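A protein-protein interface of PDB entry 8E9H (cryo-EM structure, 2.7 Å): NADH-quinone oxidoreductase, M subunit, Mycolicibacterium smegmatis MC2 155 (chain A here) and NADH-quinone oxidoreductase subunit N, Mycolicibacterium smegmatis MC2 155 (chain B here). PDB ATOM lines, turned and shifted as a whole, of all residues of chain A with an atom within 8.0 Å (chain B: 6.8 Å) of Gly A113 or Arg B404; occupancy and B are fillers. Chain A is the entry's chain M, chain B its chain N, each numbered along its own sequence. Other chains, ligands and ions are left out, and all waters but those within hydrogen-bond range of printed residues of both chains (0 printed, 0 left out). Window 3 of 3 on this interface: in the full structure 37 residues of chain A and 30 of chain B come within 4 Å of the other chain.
The guanidinium group (NE) of Arg A168 lies close to the backbone carbonyl oxygen (O) of Gly A161 (3.3 Å).
The backbone NH (N) of Arg B404 sits at hydrogen-bond distance from the backbone carbonyl oxygen (O) of Met B469 (3.4 Å).
The backbone carbonyl oxygen (O) of Gln A111 lies within hydrogen-bond range of the side-chain hydroxyl (OG) of Ser A118 (3.2 Å).
O of Phe B470 is in hydrogen-bond range of NE of Arg B404 (2.9 Å).
Among the printed residues, merely in contact across the chains: Gly A113 with Arg B404, Leu A114 with Pro B407, Ala A115 with Arg B404, Ala A115 with Pro B407, Phe A158 with Phe B470, Phe A158 with Phe B471, Gly A161 with Phe B471 and Gly A162 with Phe B471.
Hydrophobic or aromatic side chains of chain A within 4 Å of the printed part of chain B: Leu A114, Ala A115 and Phe A158.
Hydrophobic or aromatic side chains of chain B that line the printed part of chain A: Pro B407, Phe B470 and Phe B471.
Among the printed residues, 12 pairs touch across the chains.
O of Thr A112 is in hydrogen-bond range of NH1 of Arg B404 (3.1 Å).
The backbone carbonyl oxygen (O) of Phe B471 lies within hydrogen-bond range of the guanidinium group (NH2) of Arg A168 (2.9 Å).
NH2 of Arg B404 is in hydrogen-bond range of OE1 of Gln A111, 3.2 Å away.
O of Arg B404 sits at hydrogen-bond distance from N of Leu A114, at 2.7 Å.
Of the printed residues of chain B, Gly A113 touches Arg B404 (3.9 Å).
Of the printed residues of chain B, Leu A114 touches Arg B404 (2.7 Å) and Pro B407 (3.8 Å).
Ala A121 touches none of the printed residues of chain B.
Of the printed residues of chain B, Gly A161 touches Phe B471 (3.2 Å).
Of the printed residues of chain B, Gly A162 touches Phe B471.
Printed residues of chain B within 4 Å of Arg A168: Phe B471 (2.9 Å).
No residue of chain A comes within 4 Å of Gly B403.
Of the printed residues of chain A, Arg B404 touches Gln A111, Thr A112, Gly A113, Leu A114 and Ala A115.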
ATOM      1  N   ALA A  27     -17.243  -8.370  17.410  1.00  0.00           N
ATOM      2  CA  ALA A  27     -16.288  -7.277  17.564  1.00  0.00           C
ATOM      3  C   ALA A  27     -14.925  -7.641  16.993  1.00  0.00           C
ATOM      4  O   ALA A  27     -14.208  -6.777  16.475  1.00  0.00           O
ATOM      5  CB  ALA A  27     -16.161  -6.901  19.039  1.00  0.00           C
ATOM      6  N   ALA A 108     -12.580   5.122  12.479  1.00  0.00           N
ATOM      7  CA  ALA A 108     -13.248   4.675  13.693  1.00  0.00           C
ATOM      8  C   ALA A 108     -12.344   3.857  14.603  1.00  0.00           C
ATOM      9  O   ALA A 108     -12.797   3.412  15.663  1.00  0.00           O
ATOM     10  CB  ALA A 108     -14.485   3.852  13.337  1.00  0.00           C
ATOM     11  N   ARG A 110      -9.875   4.717  16.497  1.00  0.00           N
ATOM     12  CA  ARG A 110      -9.500   5.357  17.752  1.00  0.00           C
ATOM     13  C   ARG A 110     -10.618   5.352  18.786  1.00  0.00           C
ATOM     14  O   ARG A 110     -10.340   5.545  19.974  1.00  0.00           O
ATOM     15  CB  ARG A 110      -9.060   6.798  17.492  1.00  0.00           C
ATOM     16  N   GLN A 111     -11.864   5.138  18.375  1.00  0.00           N
ATOM     17  CA  GLN A 111     -12.988   5.180  19.303  1.00  0.00           C
ATOM     18  C   GLN A 111     -12.974   3.941  20.188  1.00  0.00           C
ATOM     19  O   GLN A 111     -12.832   2.818  19.695  1.00  0.00           O
ATOM     20  CB  GLN A 111     -14.306   5.281  18.541  1.00  0.00           C
ATOM     21  CG  GLN A 111     -14.635   6.680  18.045  1.00  0.00           C
ATOM     22  CD  GLN A 111     -14.868   7.662  19.177  1.00  0.00           C
ATOM     23  OE1 GLN A 111     -15.275   7.278  20.273  1.00  0.00           O
ATOM     24  NE2 GLN A 111     -14.616   8.937  18.916  1.00  0.00           N
ATOM     25  N   THR A 112     -13.124   4.149  21.492  1.00  0.00           N
ATOM     26  CA  THR A 112     -13.138   3.056  22.448  1.00  0.00           C
ATOM     27  C   THR A 112     -14.562   2.764  22.911  1.00  0.00           C
ATOM     28  O   THR A 112     -15.513   3.474  22.577  1.00  0.00           O
ATOM     29  CB  THR A 112     -12.261   3.385  23.656  1.00  0.00           C
ATOM     30  N   GLY A 113     -14.698   1.696  23.691  1.00  0.00           N
ATOM     31  CA  GLY A 113     -16.005   1.341  24.214  1.00  0.00           C
ATOM     32  C   GLY A 113     -16.921   0.838  23.116  1.00  0.00           C
ATOM     33  O   GLY A 113     -16.477   0.375  22.061  1.00  0.00           O
ATOM     34  N   LEU A 114     -18.224   0.931  23.368  1.00  0.00           N
ATOM     35  CA  LEU A 114     -19.240   0.489  22.418  1.00  0.00           C
ATOM     36  C   LEU A 114     -19.110  -1.002  22.122  1.00  0.00           C
ATOM     37  O   LEU A 114     -19.437  -1.463  21.028  1.00  0.00           O
ATOM     38  CB  LEU A 114     -19.165   1.302  21.123  1.00  0.00           C
ATOM     39  CG  LEU A 114     -20.356   1.215  20.167  1.00  0.00           C
ATOM     40  CD1 LEU A 114     -21.588   1.857  20.773  1.00  0.00           C
ATOM     41  CD2 LEU A 114     -20.014   1.869  18.847  1.00  0.00           C
ATOM     42  N   ALA A 115     -18.624  -1.767  23.101  1.00  0.00           N
ATOM     43  CA  ALA A 115     -18.494  -3.218  22.970  1.00  0.00           C
ATOM     44  C   ALA A 115     -17.590  -3.598  21.804  1.00  0.00           C
ATOM     45  O   ALA A 115     -17.702  -4.690  21.244  1.00  0.00           O
ATOM     46  CB  ALA A 115     -19.864  -3.880  22.818  1.00  0.00           C
ATOM     47  N   GLY A 116     -16.686  -2.700  21.424  1.00  0.00           N
ATOM     48  CA  GLY A 116     -15.770  -2.966  20.339  1.00  0.00           C
ATOM     49  C   GLY A 116     -16.372  -2.858  18.958  1.00  0.00           C
ATOM     50  O   GLY A 116     -15.677  -3.141  17.975  1.00  0.00           O
ATOM     51  N   ARG A 117     -17.633  -2.455  18.846  1.00  0.00           N
ATOM     52  CA  ARG A 117     -18.301  -2.342  17.558  1.00  0.00           C
ATOM     53  C   ARG A 117     -18.070  -0.995  16.894  1.00  0.00           C
ATOM     54  O   ARG A 117     -18.834  -0.629  15.994  1.00  0.00           O
ATOM     55  CB  ARG A 117     -19.804  -2.571  17.726  1.00  0.00           C
ATOM     56  CG  ARG A 117     -20.170  -3.840  18.474  1.00  0.00           C
ATOM     57  CD  ARG A 117     -19.809  -5.081  17.689  1.00  0.00           C
ATOM     58  NE  ARG A 117     -20.079  -6.294  18.454  1.00  0.00           N
ATOM     59  CZ  ARG A 117     -21.080  -7.133  18.223  1.00  0.00           C
ATOM     60  NH1 ARG A 117     -21.952  -6.926  17.249  1.00  0.00           N
ATOM     61  NH2 ARG A 117     -21.212  -8.210  18.991  1.00  0.00           N
ATOM     62  N   SER A 118     -17.044  -0.251  17.307  1.00  0.00           N
ATOM     63  CA  SER A 118     -16.847   1.090  16.771  1.00  0.00           C
ATOM     64  C   SER A 118     -16.689   1.064  15.259  1.00  0.00           C
ATOM     65  O   SER A 118     -17.365   1.813  14.545  1.00  0.00           O
ATOM     66  CB  SER A 118     -15.627   1.736  17.424  1.00  0.00           C
ATOM     67  OG  SER A 118     -15.806   1.843  18.824  1.00  0.00           O
ATOM     68  N   VAL A 119     -15.805   0.212  14.746  1.00  0.00           N
ATOM     69  CA  VAL A 119     -15.637   0.111  13.301  1.00  0.00           C
ATOM     70  C   VAL A 119     -16.918  -0.397  12.655  1.00  0.00           C
ATOM     71  O   VAL A 119     -17.375   0.134  11.635  1.00  0.00           O
ATOM     72  CB  VAL A 119     -14.441  -0.795  12.963  1.00  0.00           C
ATOM     73  CG1 VAL A 119     -14.390  -1.064  11.472  1.00  0.00           C
ATOM     74  CG2 VAL A 119     -13.150  -0.156  13.436  1.00  0.00           C
ATOM     75  N   ALA A 121     -19.933  -0.150  13.835  1.00  0.00           N
ATOM     76  CA  ALA A 121     -20.946   0.893  13.939  1.00  0.00           C
ATOM     77  C   ALA A 121     -20.740   1.964  12.878  1.00  0.00           C
ATOM     78  O   ALA A 121     -21.697   2.402  12.231  1.00  0.00           O
ATOM     79  CB  ALA A 121     -20.916   1.509  15.336  1.00  0.00           C
ATOM     80  N   PHE A 158     -25.864  10.247  14.386  1.00  0.00           N
ATOM     81  CA  PHE A 158     -24.977   9.371  15.144  1.00  0.00           C
ATOM     82  C   PHE A 158     -23.563   9.421  14.590  1.00  0.00           C
ATOM     83  O   PHE A 158     -22.590   9.495  15.347  1.00  0.00           O
ATOM     84  CB  PHE A 158     -25.503   7.940  15.112  1.00  0.00           C
ATOM     85  CG  PHE A 158     -26.569   7.667  16.122  1.00  0.00           C
ATOM     86  CD1 PHE A 158     -26.243   7.415  17.439  1.00  0.00           C
ATOM     87  CD2 PHE A 158     -27.898   7.661  15.755  1.00  0.00           C
ATOM     88  CE1 PHE A 158     -27.223   7.163  18.369  1.00  0.00           C
ATOM     89  CE2 PHE A 158     -28.881   7.410  16.680  1.00  0.00           C
ATOM     90  CZ  PHE A 158     -28.544   7.161  17.988  1.00  0.00           C
ATOM     91  N   GLY A 161     -22.018  12.784  15.884  1.00  0.00           N
ATOM     92  CA  GLY A 161     -21.810  12.810  17.315  1.00  0.00           C
ATOM     93  C   GLY A 161     -20.895  11.698  17.762  1.00  0.00           C
ATOM     94  O   GLY A 161     -19.936  11.930  18.501  1.00  0.00           O
ATOM     95  N   GLY A 162     -21.176  10.485  17.324  1.00  0.00           N
ATOM     96  CA  GLY A 162     -20.180   9.450  17.400  1.00  0.00           C
ATOM     97  C   GLY A 162     -19.068   9.724  16.419  1.00  0.00           C
ATOM     98  O   GLY A 162     -19.293  10.191  15.306  1.00  0.00           O
ATOM     99  N   PHE A 163     -17.840   9.449  16.843  1.00  0.00           N
ATOM    100  CA  PHE A 163     -16.692   9.760  16.006  1.00  0.00           C
ATOM    101  C   PHE A 163     -16.616  11.272  15.837  1.00  0.00           C
ATOM    102  O   PHE A 163     -17.469  11.998  16.356  1.00  0.00           O
ATOM    103  CB  PHE A 163     -16.815   9.054  14.654  1.00  0.00           C
ATOM    104  CG  PHE A 163     -17.322   7.642  14.761  1.00  0.00           C
ATOM    105  CD1 PHE A 163     -16.463   6.605  15.060  1.00  0.00           C
ATOM    106  CD2 PHE A 163     -18.661   7.358  14.567  1.00  0.00           C
ATOM    107  CE1 PHE A 163     -16.932   5.315  15.171  1.00  0.00           C
ATOM    108  CE2 PHE A 163     -19.132   6.072  14.677  1.00  0.00           C
ATOM    109  CZ  PHE A 163     -18.268   5.050  14.978  1.00  0.00           C
ATOM    110  N   GLY A 164     -15.619  11.762  15.121  1.00  0.00           N
ATOM    111  CA  GLY A 164     -15.501  13.194  14.948  1.00  0.00           C
ATOM    112  C   GLY A 164     -14.729  13.862  16.079  1.00  0.00           C
ATOM    113  O   GLY A 164     -14.199  13.224  16.985  1.00  0.00           O
ATOM    114  N   ARG A 168     -18.021  17.335  18.679  1.00  0.00           N
ATOM    115  CA  ARG A 168     -18.945  16.502  17.922  1.00  0.00           C
ATOM    116  C   ARG A 168     -20.357  16.573  18.479  1.00  0.00           C
ATOM    117  O   ARG A 168     -21.325  16.522  17.716  1.00  0.00           O
ATOM    118  CB  ARG A 168     -18.449  15.057  17.921  1.00  0.00           C
ATOM    119  CG  ARG A 168     -18.314  14.458  19.306  1.00  0.00           C
ATOM    120  CD  ARG A 168     -17.433  13.227  19.292  1.00  0.00           C
ATOM    121  NE  ARG A 168     -17.411  12.563  20.588  1.00  0.00           N
ATOM    122  CZ  ARG A 168     -16.542  12.826  21.553  1.00  0.00           C
ATOM    123  NH1 ARG A 168     -15.613  13.757  21.414  1.00  0.00           N
ATOM    124  NH2 ARG A 168     -16.606  12.138  22.689  1.00  0.00           N
ATOM    125  N   ALA B 400     -24.238   9.896  30.888  1.00  0.00           N
ATOM    126  CA  ALA B 400     -23.209  10.154  29.896  1.00  0.00           C
ATOM    127  C   ALA B 400     -22.445   8.878  29.583  1.00  0.00           C
ATOM    128  O   ALA B 400     -22.025   8.152  30.486  1.00  0.00           O
ATOM    129  CB  ALA B 400     -22.254  11.234  30.403  1.00  0.00           C
ATOM    130  N   GLY B 401     -22.285   8.597  28.294  1.00  0.00           N
ATOM    131  CA  GLY B 401     -21.559   7.416  27.882  1.00  0.00           C
ATOM    132  C   GLY B 401     -22.237   6.110  28.209  1.00  0.00           C
ATOM    133  O   GLY B 401     -21.622   5.055  28.044  1.00  0.00           O
ATOM    134  N   LEU B 402     -23.489   6.142  28.663  1.00  0.00           N
ATOM    135  CA  LEU B 402     -24.188   4.901  28.974  1.00  0.00           C
ATOM    136  C   LEU B 402     -24.309   4.021  27.741  1.00  0.00           C
ATOM    137  O   LEU B 402     -24.104   2.805  27.813  1.00  0.00           O
ATOM    138  CB  LEU B 402     -25.567   5.210  29.549  1.00  0.00           C
ATOM    139  CG  LEU B 402     -26.421   4.002  29.922  1.00  0.00           C
ATOM    140  CD1 LEU B 402     -25.851   3.301  31.138  1.00  0.00           C
ATOM    141  CD2 LEU B 402     -27.849   4.436  30.173  1.00  0.00           C
ATOM    142  N   GLY B 403     -24.644   4.616  26.597  1.00  0.00           N
ATOM    143  CA  GLY B 403     -24.732   3.840  25.375  1.00  0.00           C
ATOM    144  C   GLY B 403     -23.424   3.180  25.007  1.00  0.00           C
ATOM    145  O   GLY B 403     -23.409   2.032  24.556  1.00  0.00           O
ATOM    146  N   ARG B 404     -22.307   3.883  25.201  1.00  0.00           N
ATOM    147  CA  ARG B 404     -21.013   3.299  24.883  1.00  0.00           C
ATOM    148  C   ARG B 404     -20.718   2.091  25.757  1.00  0.00           C
ATOM    149  O   ARG B 404     -20.128   1.114  25.284  1.00  0.00           O
ATOM    150  CB  ARG B 404     -19.916   4.348  25.036  1.00  0.00           C
ATOM    151  CG  ARG B 404     -20.024   5.481  24.034  1.00  0.00           C
ATOM    152  CD  ARG B 404     -18.681   6.128  23.751  1.00  0.00           C
ATOM    153  NE  ARG B 404     -18.639   6.708  22.414  1.00  0.00           N
ATOM    154  CZ  ARG B 404     -18.375   6.024  21.309  1.00  0.00           C
ATOM    155  NH1 ARG B 404     -18.117   4.728  21.340  1.00  0.00           N
ATOM    156  NH2 ARG B 404     -18.372   6.658  20.140  1.00  0.00           N
ATOM    157  N   ARG B 405     -21.114   2.136  27.028  1.00  0.00           N
ATOM    158  CA  ARG B 405     -20.915   0.989  27.905  1.00  0.00           C
ATOM    159  C   ARG B 405     -21.861  -0.153  27.558  1.00  0.00           C
ATOM    160  O   ARG B 405     -21.467  -1.322  27.599  1.00  0.00           O
ATOM    161  CB  ARG B 405     -21.111   1.411  29.360  1.00  0.00           C
ATOM    162  CG  ARG B 405     -19.973   2.238  29.921  1.00  0.00           C
ATOM    163  CD  ARG B 405     -20.428   3.055  31.114  1.00  0.00           C
ATOM    164  NE  ARG B 405     -20.959   2.215  32.180  1.00  0.00           N
ATOM    165  CZ  ARG B 405     -20.216   1.505  33.018  1.00  0.00           C
ATOM    166  NH1 ARG B 405     -18.895   1.509  32.945  1.00  0.00           N
ATOM    167  NH2 ARG B 405     -20.814   0.771  33.951  1.00  0.00           N
ATOM    168  N   TYR B 406     -23.107   0.165  27.211  1.00  0.00           N
ATOM    169  CA  TYR B 406     -24.149  -0.829  26.960  1.00  0.00           C
ATOM    170  C   TYR B 406     -24.791  -0.523  25.615  1.00  0.00           C
ATOM    171  O   TYR B 406     -25.894   0.035  25.548  1.00  0.00           O
ATOM    172  CB  TYR B 406     -25.174  -0.836  28.092  1.00  0.00           C
ATOM    173  CG  TYR B 406     -24.541  -1.040  29.444  1.00  0.00           C
ATOM    174  CD1 TYR B 406     -23.931  -2.242  29.765  1.00  0.00           C
ATOM    175  CD2 TYR B 406     -24.538  -0.033  30.393  1.00  0.00           C
ATOM    176  CE1 TYR B 406     -23.346  -2.437  30.995  1.00  0.00           C
ATOM    177  CE2 TYR B 406     -23.953  -0.219  31.627  1.00  0.00           C
ATOM    178  CZ  TYR B 406     -23.357  -1.423  31.922  1.00  0.00           C
ATOM    179  OH  TYR B 406     -22.773  -1.618  33.149  1.00  0.00           O
ATOM    180  N   PRO B 407     -24.122  -0.876  24.516  1.00  0.00           N
ATOM    181  CA  PRO B 407     -24.639  -0.480  23.198  1.00  0.00           C
ATOM    182  C   PRO B 407     -26.026  -1.007  22.891  1.00  0.00           C
ATOM    183  O   PRO B 407     -26.804  -0.305  22.241  1.00  0.00           O
ATOM    184  CB  PRO B 407     -23.590  -1.045  22.230  1.00  0.00           C
ATOM    185  CG  PRO B 407     -22.895  -2.109  22.991  1.00  0.00           C
ATOM    186  CD  PRO B 407     -22.881  -1.657  24.409  1.00  0.00           C
ATOM    187  N   GLY B 410     -28.512   0.872  24.968  1.00  0.00           N
ATOM    188  CA  GLY B 410     -28.457   2.242  24.501  1.00  0.00           C
ATOM    189  C   GLY B 410     -29.182   2.433  23.185  1.00  0.00           C
ATOM    190  O   GLY B 410     -29.910   3.409  23.002  1.00  0.00           O
ATOM    191  N   LEU B 468     -25.807  12.484  25.371  1.00  0.00           N
ATOM    192  CA  LEU B 468     -25.144  12.036  26.589  1.00  0.00           C
ATOM    193  C   LEU B 468     -24.812  10.553  26.499  1.00  0.00           C
ATOM    194  O   LEU B 468     -23.719  10.116  26.869  1.00  0.00           O
ATOM    195  CB  LEU B 468     -26.034  12.318  27.796  1.00  0.00           C
ATOM    196  CG  LEU B 468     -26.147  13.792  28.175  1.00  0.00           C
ATOM    197  CD1 LEU B 468     -27.463  14.050  28.879  1.00  0.00           C
ATOM    198  CD2 LEU B 468     -24.981  14.210  29.046  1.00  0.00           C
ATOM    199  N   MET B 469     -25.748   9.769  25.974  1.00  0.00           N
ATOM    200  CA  MET B 469     -25.635   8.319  26.021  1.00  0.00           C
ATOM    201  C   MET B 469     -24.492   7.812  25.152  1.00  0.00           C
ATOM    202  O   MET B 469     -23.770   6.891  25.548  1.00  0.00           O
ATOM    203  CB  MET B 469     -26.966   7.719  25.586  1.00  0.00           C
ATOM    204  CG  MET B 469     -27.811   7.236  26.736  1.00  0.00           C
ATOM    205  SD  MET B 469     -29.413   6.660  26.172  1.00  0.00           S
ATOM    206  CE  MET B 469     -28.914   5.346  25.085  1.00  0.00           C
ATOM    207  N   PHE B 470     -24.311   8.392  23.970  1.00  0.00           N
ATOM    208  CA  PHE B 470     -23.343   7.884  23.003  1.00  0.00           C
ATOM    209  C   PHE B 470     -22.167   8.813  22.755  1.00  0.00           C
ATOM    210  O   PHE B 470     -21.029   8.350  22.703  1.00  0.00           O
ATOM    211  CB  PHE B 470     -24.039   7.607  21.670  1.00  0.00           C
ATOM    212  CG  PHE B 470     -24.831   6.339  21.659  1.00  0.00           C
ATOM    213  CD1 PHE B 470     -24.221   5.130  21.393  1.00  0.00           C
ATOM    214  CD2 PHE B 470     -26.185   6.354  21.926  1.00  0.00           C
ATOM    215  CE1 PHE B 470     -24.947   3.964  21.385  1.00  0.00           C
ATOM    216  CE2 PHE B 470     -26.914   5.188  21.920  1.00  0.00           C
ATOM    217  CZ  PHE B 470     -26.295   3.992  21.650  1.00  0.00           C
ATOM    218  N   PHE B 471     -22.405  10.109  22.593  1.00  0.00           N
ATOM    219  CA  PHE B 471     -21.356  11.026  22.176  1.00  0.00           C
ATOM    220  C   PHE B 471     -20.473  11.490  23.324  1.00  0.00           C
ATOM    221  O   PHE B 471     -19.440  12.120  23.073  1.00  0.00           O
ATOM    222  CB  PHE B 471     -21.972  12.254  21.500  1.00  0.00           C
ATOM    223  CG  PHE B 471     -22.999  11.926  20.455  1.00  0.00           C
ATOM    224  CD1 PHE B 471     -23.037  10.680  19.853  1.00  0.00           C
ATOM    225  CD2 PHE B 471     -23.936  12.866  20.081  1.00  0.00           C
ATOM    226  CE1 PHE B 471     -23.983  10.388  18.901  1.00  0.00           C
ATOM    227  CE2 PHE B 471     -24.884  12.576  19.133  1.00  0.00           C
ATOM    228  CZ  PHE B 471     -24.908  11.335  18.540  1.00  0.00           C
ATOM    229  N   THR B 472     -20.844  11.198  24.564  1.00  0.00           N
ATOM    230  CA  THR B 472     -20.098  11.647  25.729  1.00  0.00           C
ATOM    231  C   THR B 472     -19.341  10.483  26.352  1.00  0.00           C
ATOM    232  O   THR B 472     -19.820   9.345  26.350  1.00  0.00           O
ATOM    233  CB  THR B 472     -21.034  12.267  26.767  1.00  0.00           C
ATOM    234  OG1 THR B 472     -21.900  13.212  26.129  1.00  0.00           O
ATOM    235  CG2 THR B 472     -20.240  12.970  27.852  1.00  0.00           C
ATOM    236  N   GLU B 473     -18.154  10.772  26.874  1.00  0.00           N
ATOM    237  CA  GLU B 473     -17.380   9.749  27.553  1.00  0.00           C
ATOM    238  C   GLU B 473     -18.001   9.440  28.916  1.00  0.00           C
ATOM    239  O   GLU B 473     -18.436  10.350  29.626  1.00  0.00           O
ATOM    240  CB  GLU B 473     -15.936  10.204  27.735  1.00  0.00           C
ATOM    241  N   PRO B 474     -18.048   8.171  29.312  1.00  0.00           N
ATOM    242  CA  PRO B 474     -18.687   7.821  30.584  1.00  0.00           C
ATOM    243  C   PRO B 474     -17.973   8.478  31.750  1.00  0.00           C
ATOM    244  O   PRO B 474     -16.746   8.649  31.717  1.00  0.00           O
ATOM    245  CB  PRO B 474     -18.558   6.291  30.647  1.00  0.00           C
ATOM    246  CG  PRO B 474     -18.232   5.858  29.276  1.00  0.00           C
ATOM    247  CD  PRO B 474     -17.505   6.984  28.631  1.00  0.00           C
